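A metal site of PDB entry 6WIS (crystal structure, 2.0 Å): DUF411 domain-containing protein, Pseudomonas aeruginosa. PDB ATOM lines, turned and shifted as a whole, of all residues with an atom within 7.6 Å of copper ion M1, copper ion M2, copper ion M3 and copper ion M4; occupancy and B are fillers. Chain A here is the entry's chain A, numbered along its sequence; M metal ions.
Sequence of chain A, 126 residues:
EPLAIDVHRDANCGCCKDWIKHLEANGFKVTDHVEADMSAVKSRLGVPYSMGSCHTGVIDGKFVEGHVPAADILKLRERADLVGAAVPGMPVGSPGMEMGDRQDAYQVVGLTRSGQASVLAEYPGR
The side-chain sulfur (SG) of Cys 16 is bound to copper ion M2 (2.2 Å).
A ring nitrogen (ND1) of His 55 is bound to copper ion M2.
The side-chain sulfur (SG) of Cys 54 binds copper ion M2, 2.3 Å away.
Copper ion M2 has three donor atoms within binding distance.
Copper ion M4 is bound by SG of Cys 15, SD of Met 97 and SD of Met 90.
Copper ion M4 has three donor atoms within binding distance.
Within 4 Å of copper ion M3: Cys 13, Cys 15, Cys 16, Cys 54, His 67 and Met 90.
The nearest printed residue that does not touch copper ion M3 is Met 97 (4.3 Å).
Copper ion M1 is bound by the backbone nitrogen of Cys 16 (2.1 Å), the side-chain sulfur of Cys 16 (2.2 Å), the side-chain sulfur of Cys 13 (2.3 Å) and the side-chain sulfur of Cys 15 (2.3 Å).
Of the 29 residues printed, 4 come within 4 Å of copper ion M2.
The nearest printed residue that does not touch copper ion M2 is Cys 13 (4.3 Å).
Three residues have an atom within 4 Å of copper ion M4: Cys 15, Met 90 and Met 97.
The nearest printed residue that does not touch copper ion M4 is His 67 (4.3 Å).
A ring nitrogen (ND1) of His 67 sits at hydrogen-bond distance from the backbone carbonyl oxygen of Pro 95.
O of Gly 66 sits at hydrogen-bond distance from NE2 of His 55 (2.7 Å).
The side-chain sulfur of Cys 54 lies close to the side-chain hydroxyl of Ser 53.
The backbone NH (N) of Asp 10 sits at hydrogen-bond distance from the backbone carbonyl oxygen (O) of Cys 54 (3.0 Å).
Copper ion M3 is bound by a ring nitrogen (NE2) of His 67, 2.1 Å away.
SG of Cys 15 binds copper ion M3, 2.3 Å away.
SG of Cys 54 is bound to copper ion M3, 2.3 Å away.
Of the 29 residues printed, 4 come within 4 Å of copper ion M1.
The nearest printed residue that does not touch copper ion M1 is Gly 14 (4.1 Å).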
ATOM      1  N   VAL A   7       0.076  29.669 -16.197  1.00  0.00           N
ATOM      2  CA  VAL A   7       1.328  28.916 -16.338  1.00  0.00           C
ATOM      3  C   VAL A   7       2.503  29.871 -16.428  1.00  0.00           C
ATOM      4  O   VAL A   7       2.536  30.772 -17.286  1.00  0.00           O
ATOM      5  CB  VAL A   7       1.275  27.984 -17.553  1.00  0.00           C
ATOM      6  CG1 VAL A   7       2.604  27.198 -17.675  1.00  0.00           C
ATOM      7  CG2 VAL A   7       0.082  27.015 -17.414  1.00  0.00           C
ATOM      8  N   HIS A   8       3.486  29.675 -15.544  1.00  0.00           N
ATOM      9  CA  HIS A   8       4.787  30.332 -15.621  1.00  0.00           C
ATOM     10  C   HIS A   8       5.765  29.307 -16.183  1.00  0.00           C
ATOM     11  O   HIS A   8       5.948  28.240 -15.580  1.00  0.00           O
ATOM     12  CB  HIS A   8       5.273  30.809 -14.241  1.00  0.00           C
ATOM     13  CG  HIS A   8       4.194  31.376 -13.381  1.00  0.00           C
ATOM     14  ND1 HIS A   8       4.104  32.724 -13.083  1.00  0.00           N
ATOM     15  CD2 HIS A   8       3.164  30.785 -12.732  1.00  0.00           C
ATOM     16  CE1 HIS A   8       3.069  32.935 -12.307  1.00  0.00           C
ATOM     17  NE2 HIS A   8       2.477  31.775 -12.076  1.00  0.00           N
ATOM     18  N   ARG A   9       6.369  29.607 -17.334  1.00  0.00           N
ATOM     19  CA  ARG A   9       7.166  28.581 -18.020  1.00  0.00           C
ATOM     20  C   ARG A   9       8.559  29.078 -18.361  1.00  0.00           C
ATOM     21  O   ARG A   9       8.795  30.266 -18.589  1.00  0.00           O
ATOM     22  CB  ARG A   9       6.450  28.091 -19.290  1.00  0.00           C
ATOM     23  CG  ARG A   9       6.146  29.173 -20.318  1.00  0.00           C
ATOM     24  CD  ARG A   9       5.578  28.575 -21.607  1.00  0.00           C
ATOM     25  NE  ARG A   9       4.999  29.580 -22.490  1.00  0.00           N
ATOM     26  CZ  ARG A   9       5.611  30.118 -23.544  1.00  0.00           C
ATOM     27  NH1 ARG A   9       6.847  29.766 -23.880  1.00  0.00           N
ATOM     28  NH2 ARG A   9       4.970  31.013 -24.293  1.00  0.00           N
ATOM     29  N   ASP A  10       9.488  28.122 -18.404  1.00  0.00           N
ATOM     30  CA  ASP A  10      10.878  28.373 -18.790  1.00  0.00           C
ATOM     31  C   ASP A  10      10.957  28.993 -20.175  1.00  0.00           C
ATOM     32  O   ASP A  10      10.169  28.670 -21.072  1.00  0.00           O
ATOM     33  CB  ASP A  10      11.669  27.073 -18.770  1.00  0.00           C
ATOM     34  CG  ASP A  10      12.179  26.732 -17.400  1.00  0.00           C
ATOM     35  OD1 ASP A  10      11.962  27.532 -16.459  1.00  0.00           O
ATOM     36  OD2 ASP A  10      12.819  25.673 -17.250  1.00  0.00           O
ATOM     37  N   ALA A  11      11.900  29.909 -20.352  1.00  0.00           N
ATOM     38  CA  ALA A  11      12.129  30.454 -21.689  1.00  0.00           C
ATOM     39  C   ALA A  11      12.630  29.367 -22.618  1.00  0.00           C
ATOM     40  O   ALA A  11      13.379  28.466 -22.200  1.00  0.00           O
ATOM     41  CB  ALA A  11      13.136  31.615 -21.637  1.00  0.00           C
ATOM     42  N   ASN A  12      12.203  29.424 -23.890  1.00  0.00           N
ATOM     43  CA  ASN A  12      12.755  28.599 -24.982  1.00  0.00           C
ATOM     44  C   ASN A  12      12.550  27.103 -24.724  1.00  0.00           C
ATOM     45  O   ASN A  12      13.413  26.284 -25.021  1.00  0.00           O
ATOM     46  CB  ASN A  12      14.243  28.902 -25.222  1.00  0.00           C
ATOM     47  CG  ASN A  12      14.747  28.267 -26.526  1.00  0.00           C
ATOM     48  OD1 ASN A  12      14.132  28.440 -27.585  1.00  0.00           O
ATOM     49  ND2 ASN A  12      15.829  27.496 -26.445  1.00  0.00           N
ATOM     50  N   CYS A  13      11.399  26.749 -24.157  1.00  0.00           N
ATOM     51  CA  CYS A  13      11.098  25.376 -23.772  1.00  0.00           C
ATOM     52  C   CYS A  13       9.861  24.950 -24.562  1.00  0.00           C
ATOM     53  O   CYS A  13       8.760  25.472 -24.322  1.00  0.00           O
ATOM     54  CB  CYS A  13      10.885  25.271 -22.261  1.00  0.00           C
ATOM     55  SG  CYS A  13      10.887  23.593 -21.594  1.00  0.00           S
ATOM     56  N   GLY A  14      10.047  24.040 -25.511  1.00  0.00           N
ATOM     57  CA  GLY A  14       8.985  23.642 -26.415  1.00  0.00           C
ATOM     58  C   GLY A  14       7.952  22.743 -25.758  1.00  0.00           C
ATOM     59  O   GLY A  14       6.761  22.871 -26.055  1.00  0.00           O
ATOM     60  N   CYS A  15       8.405  21.873 -24.845  1.00  0.00           N
ATOM     61  CA  CYS A  15       7.493  20.938 -24.175  1.00  0.00           C
ATOM     62  C   CYS A  15       6.446  21.660 -23.326  1.00  0.00           C
ATOM     63  O   CYS A  15       5.296  21.208 -23.253  1.00  0.00           O
ATOM     64  CB  CYS A  15       8.287  19.951 -23.314  1.00  0.00           C
ATOM     65  SG  CYS A  15       9.514  20.838 -22.322  1.00  0.00           S
ATOM     66  N   CYS A  16       6.818  22.768 -22.672  1.00  0.00           N
ATOM     67  CA  CYS A  16       5.827  23.545 -21.911  1.00  0.00           C
ATOM     68  C   CYS A  16       4.673  23.991 -22.790  1.00  0.00           C
ATOM     69  O   CYS A  16       3.512  23.920 -22.381  1.00  0.00           O
ATOM     70  CB  CYS A  16       6.466  24.779 -21.259  1.00  0.00           C
ATOM     71  SG  CYS A  16       8.030  24.550 -20.348  1.00  0.00           S
ATOM     72  N   LYS A  17       4.976  24.482 -23.993  1.00  0.00           N
ATOM     73  CA  LYS A  17       3.938  24.929 -24.915  1.00  0.00           C
ATOM     74  C   LYS A  17       3.082  23.772 -25.408  1.00  0.00           C
ATOM     75  O   LYS A  17       1.875  23.949 -25.621  1.00  0.00           O
ATOM     76  CB  LYS A  17       4.584  25.651 -26.117  1.00  0.00           C
ATOM     77  CG  LYS A  17       5.239  27.007 -25.768  1.00  0.00           C
ATOM     78  CD  LYS A  17       6.058  27.574 -26.943  1.00  0.00           C
ATOM     79  N   ASP A  18       3.686  22.597 -25.588  1.00  0.00           N
ATOM     80  CA  ASP A  18       2.929  21.407 -25.978  1.00  0.00           C
ATOM     81  C   ASP A  18       2.004  20.970 -24.845  1.00  0.00           C
ATOM     82  O   ASP A  18       0.838  20.633 -25.074  1.00  0.00           O
ATOM     83  CB  ASP A  18       3.911  20.286 -26.361  1.00  0.00           C
ATOM     84  CG  ASP A  18       3.226  19.055 -26.990  1.00  0.00           C
ATOM     85  OD1 ASP A  18       2.101  19.130 -27.500  1.00  0.00           O
ATOM     86  OD2 ASP A  18       3.834  17.981 -26.998  1.00  0.00           O
ATOM     87  N   TRP A  19       2.505  20.976 -23.598  1.00  0.00           N
ATOM     88  CA  TRP A  19       1.646  20.664 -22.453  1.00  0.00           C
ATOM     89  C   TRP A  19       0.456  21.625 -22.373  1.00  0.00           C
ATOM     90  O   TRP A  19      -0.678  21.190 -22.128  1.00  0.00           O
ATOM     91  CB  TRP A  19       2.484  20.716 -21.181  1.00  0.00           C
ATOM     92  CG  TRP A  19       1.791  20.425 -19.929  1.00  0.00           C
ATOM     93  CD1 TRP A  19       1.387  19.198 -19.487  1.00  0.00           C
ATOM     94  CD2 TRP A  19       1.447  21.356 -18.894  1.00  0.00           C
ATOM     95  NE1 TRP A  19       0.807  19.314 -18.226  1.00  0.00           N
ATOM     96  CE2 TRP A  19       0.854  20.633 -17.837  1.00  0.00           C
ATOM     97  CE3 TRP A  19       1.609  22.746 -18.758  1.00  0.00           C
ATOM     98  CZ2 TRP A  19       0.416  21.248 -16.660  1.00  0.00           C
ATOM     99  CZ3 TRP A  19       1.169  23.360 -17.565  1.00  0.00           C
ATOM    100  CH2 TRP A  19       0.573  22.617 -16.544  1.00  0.00           C
ATOM    101  N   MET A  38      11.975  32.460 -11.828  1.00  0.00           N
ATOM    102  CA  MET A  38      11.339  31.179 -11.590  1.00  0.00           C
ATOM    103  C   MET A  38      11.613  30.660 -10.167  1.00  0.00           C
ATOM    104  O   MET A  38      10.743  30.017  -9.571  1.00  0.00           O
ATOM    105  CB  MET A  38      11.788  30.150 -12.631  1.00  0.00           C
ATOM    106  CG  MET A  38      11.070  28.817 -12.467  1.00  0.00           C
ATOM    107  SD  MET A  38       9.148  29.003 -12.907  1.00  0.00           S
ATOM    108  CE  MET A  38       9.303  28.677 -14.803  1.00  0.00           C
ATOM    109  N   SER A  53      10.463  21.497 -12.024  1.00  0.00           N
ATOM    110  CA  SER A  53      10.368  21.059 -13.413  1.00  0.00           C
ATOM    111  C   SER A  53      10.574  22.301 -14.248  1.00  0.00           C
ATOM    112  O   SER A  53      11.121  23.310 -13.779  1.00  0.00           O
ATOM    113  CB  SER A  53       9.033  20.330 -13.639  1.00  0.00           C
ATOM    114  OG  SER A  53       8.950  19.744 -14.928  1.00  0.00           O
ATOM    115  N   CYS A  54      10.122  22.257 -15.509  1.00  0.00           N
ATOM    116  CA  CYS A  54      10.349  23.322 -16.486  1.00  0.00           C
ATOM    117  C   CYS A  54       9.258  24.386 -16.496  1.00  0.00           C
ATOM    118  O   CYS A  54       9.409  25.430 -17.163  1.00  0.00           O
ATOM    119  CB  CYS A  54      10.448  22.685 -17.878  1.00  0.00           C
ATOM    120  SG  CYS A  54       9.071  21.486 -18.122  1.00  0.00           S
ATOM    121  N   HIS A  55       8.132  24.156 -15.816  1.00  0.00           N
ATOM    122  CA  HIS A  55       7.082  25.161 -15.756  1.00  0.00           C
ATOM    123  C   HIS A  55       6.288  24.966 -14.469  1.00  0.00           C
ATOM    124  O   HIS A  55       6.320  23.891 -13.868  1.00  0.00           O
ATOM    125  CB  HIS A  55       6.149  25.082 -16.978  1.00  0.00           C
ATOM    126  CG  HIS A  55       5.366  23.795 -17.046  1.00  0.00           C
ATOM    127  ND1 HIS A  55       5.627  22.801 -17.963  1.00  0.00           N
ATOM    128  CD2 HIS A  55       4.324  23.349 -16.298  1.00  0.00           C
ATOM    129  CE1 HIS A  55       4.781  21.792 -17.782  1.00  0.00           C
ATOM    130  NE2 HIS A  55       3.992  22.094 -16.755  1.00  0.00           N
ATOM    131  N   THR A  56       5.550  25.994 -14.067  1.00  0.00           N
ATOM    132  CA  THR A  56       4.738  25.937 -12.852  1.00  0.00           C
ATOM    133  C   THR A  56       3.370  26.533 -13.173  1.00  0.00           C
ATOM    134  O   THR A  56       3.284  27.694 -13.586  1.00  0.00           O
ATOM    135  CB  THR A  56       5.374  26.719 -11.690  1.00  0.00           C
ATOM    136  OG1 THR A  56       6.715  26.246 -11.467  1.00  0.00           O
ATOM    137  CG2 THR A  56       4.542  26.516 -10.414  1.00  0.00           C
ATOM    138  N   GLU A  65       3.246  21.410 -10.910  1.00  0.00           N
ATOM    139  CA  GLU A  65       4.661  21.505 -11.265  1.00  0.00           C
ATOM    140  C   GLU A  65       4.955  20.484 -12.355  1.00  0.00           C
ATOM    141  O   GLU A  65       4.801  19.274 -12.136  1.00  0.00           O
ATOM    142  CB  GLU A  65       5.543  21.265 -10.042  1.00  0.00           C
ATOM    143  CG  GLU A  65       7.039  21.434 -10.316  1.00  0.00           C
ATOM    144  CD  GLU A  65       7.427  22.889 -10.601  1.00  0.00           C
ATOM    145  OE1 GLU A  65       6.571  23.764 -10.351  1.00  0.00           O
ATOM    146  OE2 GLU A  65       8.572  23.156 -11.070  1.00  0.00           O
ATOM    147  N   GLY A  66       5.342  20.950 -13.521  1.00  0.00           N
ATOM    148  CA  GLY A  66       5.722  20.013 -14.557  1.00  0.00           C
ATOM    149  C   GLY A  66       4.557  19.408 -15.347  1.00  0.00           C
ATOM    150  O   GLY A  66       3.416  19.899 -15.378  1.00  0.00           O
ATOM    151  N   HIS A  67       4.889  18.316 -16.024  1.00  0.00           N
ATOM    152  CA  HIS A  67       4.011  17.721 -17.038  1.00  0.00           C
ATOM    153  C   HIS A  67       2.951  16.802 -16.398  1.00  0.00           C
ATOM    154  O   HIS A  67       2.870  15.607 -16.675  1.00  0.00           O
ATOM    155  CB  HIS A  67       4.870  17.005 -18.063  1.00  0.00           C
ATOM    156  CG  HIS A  67       5.662  17.942 -18.918  1.00  0.00           C
ATOM    157  ND1 HIS A  67       5.197  18.417 -20.130  1.00  0.00           N
ATOM    158  CD2 HIS A  67       6.849  18.563 -18.720  1.00  0.00           C
ATOM    159  CE1 HIS A  67       6.067  19.267 -20.638  1.00  0.00           C
ATOM    160  NE2 HIS A  67       7.080  19.380 -19.799  1.00  0.00           N
ATOM    161  N   GLY A  89      11.219  17.098 -12.891  1.00  0.00           N
ATOM    162  CA  GLY A  89      11.997  16.846 -14.090  1.00  0.00           C
ATOM    163  C   GLY A  89      11.133  16.910 -15.349  1.00  0.00           C
ATOM    164  O   GLY A  89      10.134  17.636 -15.429  1.00  0.00           O
ATOM    165  N   MET A  90      11.542  16.133 -16.357  1.00  0.00           N
ATOM    166  CA  MET A  90      10.780  16.075 -17.595  1.00  0.00           C
ATOM    167  C   MET A  90      10.830  14.673 -18.155  1.00  0.00           C
ATOM    168  O   MET A  90      11.586  14.416 -19.089  1.00  0.00           O
ATOM    169  CB  MET A  90      11.334  17.072 -18.629  1.00  0.00           C
ATOM    170  CG  MET A  90      11.363  18.538 -18.217  1.00  0.00           C
ATOM    171  SD  MET A  90      12.101  19.725 -19.619  1.00  0.00           S
ATOM    172  CE  MET A  90      13.881  18.931 -19.816  1.00  0.00           C
ATOM    173  N   PRO A  91      10.029  13.778 -17.583  1.00  0.00           N
ATOM    174  CA  PRO A  91      10.052  12.371 -18.041  1.00  0.00           C
ATOM    175  C   PRO A  91       9.473  12.250 -19.431  1.00  0.00           C
ATOM    176  O   PRO A  91       8.408  12.804 -19.727  1.00  0.00           O
ATOM    177  CB  PRO A  91       9.192  11.641 -17.008  1.00  0.00           C
ATOM    178  CG  PRO A  91       8.349  12.718 -16.382  1.00  0.00           C
ATOM    179  CD  PRO A  91       9.162  13.973 -16.406  1.00  0.00           C
ATOM    180  N   SER A  94       5.440  11.767 -20.727  1.00  0.00           N
ATOM    181  CA  SER A  94       4.429  12.551 -20.044  1.00  0.00           C
ATOM    182  C   SER A  94       3.814  13.552 -21.020  1.00  0.00           C
ATOM    183  O   SER A  94       4.404  13.843 -22.068  1.00  0.00           O
ATOM    184  CB  SER A  94       5.037  13.257 -18.822  1.00  0.00           C
ATOM    185  OG  SER A  94       6.016  14.221 -19.194  1.00  0.00           O
ATOM    186  N   PRO A  95       2.617  14.069 -20.723  1.00  0.00           N
ATOM    187  CA  PRO A  95       1.931  14.929 -21.708  1.00  0.00           C
ATOM    188  C   PRO A  95       2.717  16.199 -21.998  1.00  0.00           C
ATOM    189  O   PRO A  95       3.132  16.918 -21.092  1.00  0.00           O
ATOM    190  CB  PRO A  95       0.584  15.244 -21.051  1.00  0.00           C
ATOM    191  CG  PRO A  95       0.426  14.267 -19.918  1.00  0.00           C
ATOM    192  CD  PRO A  95       1.795  13.800 -19.527  1.00  0.00           C
ATOM    193  N   GLY A  96       2.906  16.476 -23.287  1.00  0.00           N
ATOM    194  CA  GLY A  96       3.765  17.567 -23.711  1.00  0.00           C
ATOM    195  C   GLY A  96       5.219  17.200 -23.839  1.00  0.00           C
ATOM    196  O   GLY A  96       5.986  17.977 -24.424  1.00  0.00           O
ATOM    197  N   MET A  97       5.622  16.033 -23.355  1.00  0.00           N
ATOM    198  CA  MET A  97       6.986  15.503 -23.450  1.00  0.00           C
ATOM    199  C   MET A  97       6.962  14.174 -24.223  1.00  0.00           C
ATOM    200  O   MET A  97       7.871  13.374 -24.132  1.00  0.00           O
ATOM    201  CB  MET A  97       7.599  15.289 -22.061  1.00  0.00           C
ATOM    202  CG  MET A  97       8.364  16.540 -21.426  1.00  0.00           C
ATOM    203  SD  MET A  97       9.908  17.130 -22.516  1.00  0.00           S
ATOM    204  CE  MET A  97      10.894  15.425 -22.336  1.00  0.00           C
ATOM    205  N   MET A  99       7.392  11.402 -26.978  1.00  0.00           N
ATOM    206  CA  MET A  99       8.267  11.215 -28.136  1.00  0.00           C
ATOM    207  C   MET A  99       8.254   9.740 -28.587  1.00  0.00           C
ATOM    208  O   MET A  99       9.249   9.031 -28.419  1.00  0.00           O
ATOM    209  CB  MET A  99       9.700  11.642 -27.794  1.00  0.00           C
ATOM    210  CG  MET A  99       9.824  13.103 -27.383  1.00  0.00           C
ATOM    211  SD  MET A  99      11.590  13.687 -26.942  1.00  0.00           S
ATOM    212  CE  MET A  99      11.080  15.431 -26.326  1.00  0.00           C
HETATM  213 CU    CU M   1       8.727  22.970 -21.785  1.00  0.00          CU
HETATM  214 CU    CU M   2       7.563  22.951 -18.959  1.00  0.00          CU
HETATM  215 CU    CU M   3       8.704  20.654 -20.218  1.00  0.00          CU
HETATM  216 CU    CU M   4      10.973  19.116 -21.672  1.00  0.00          CU
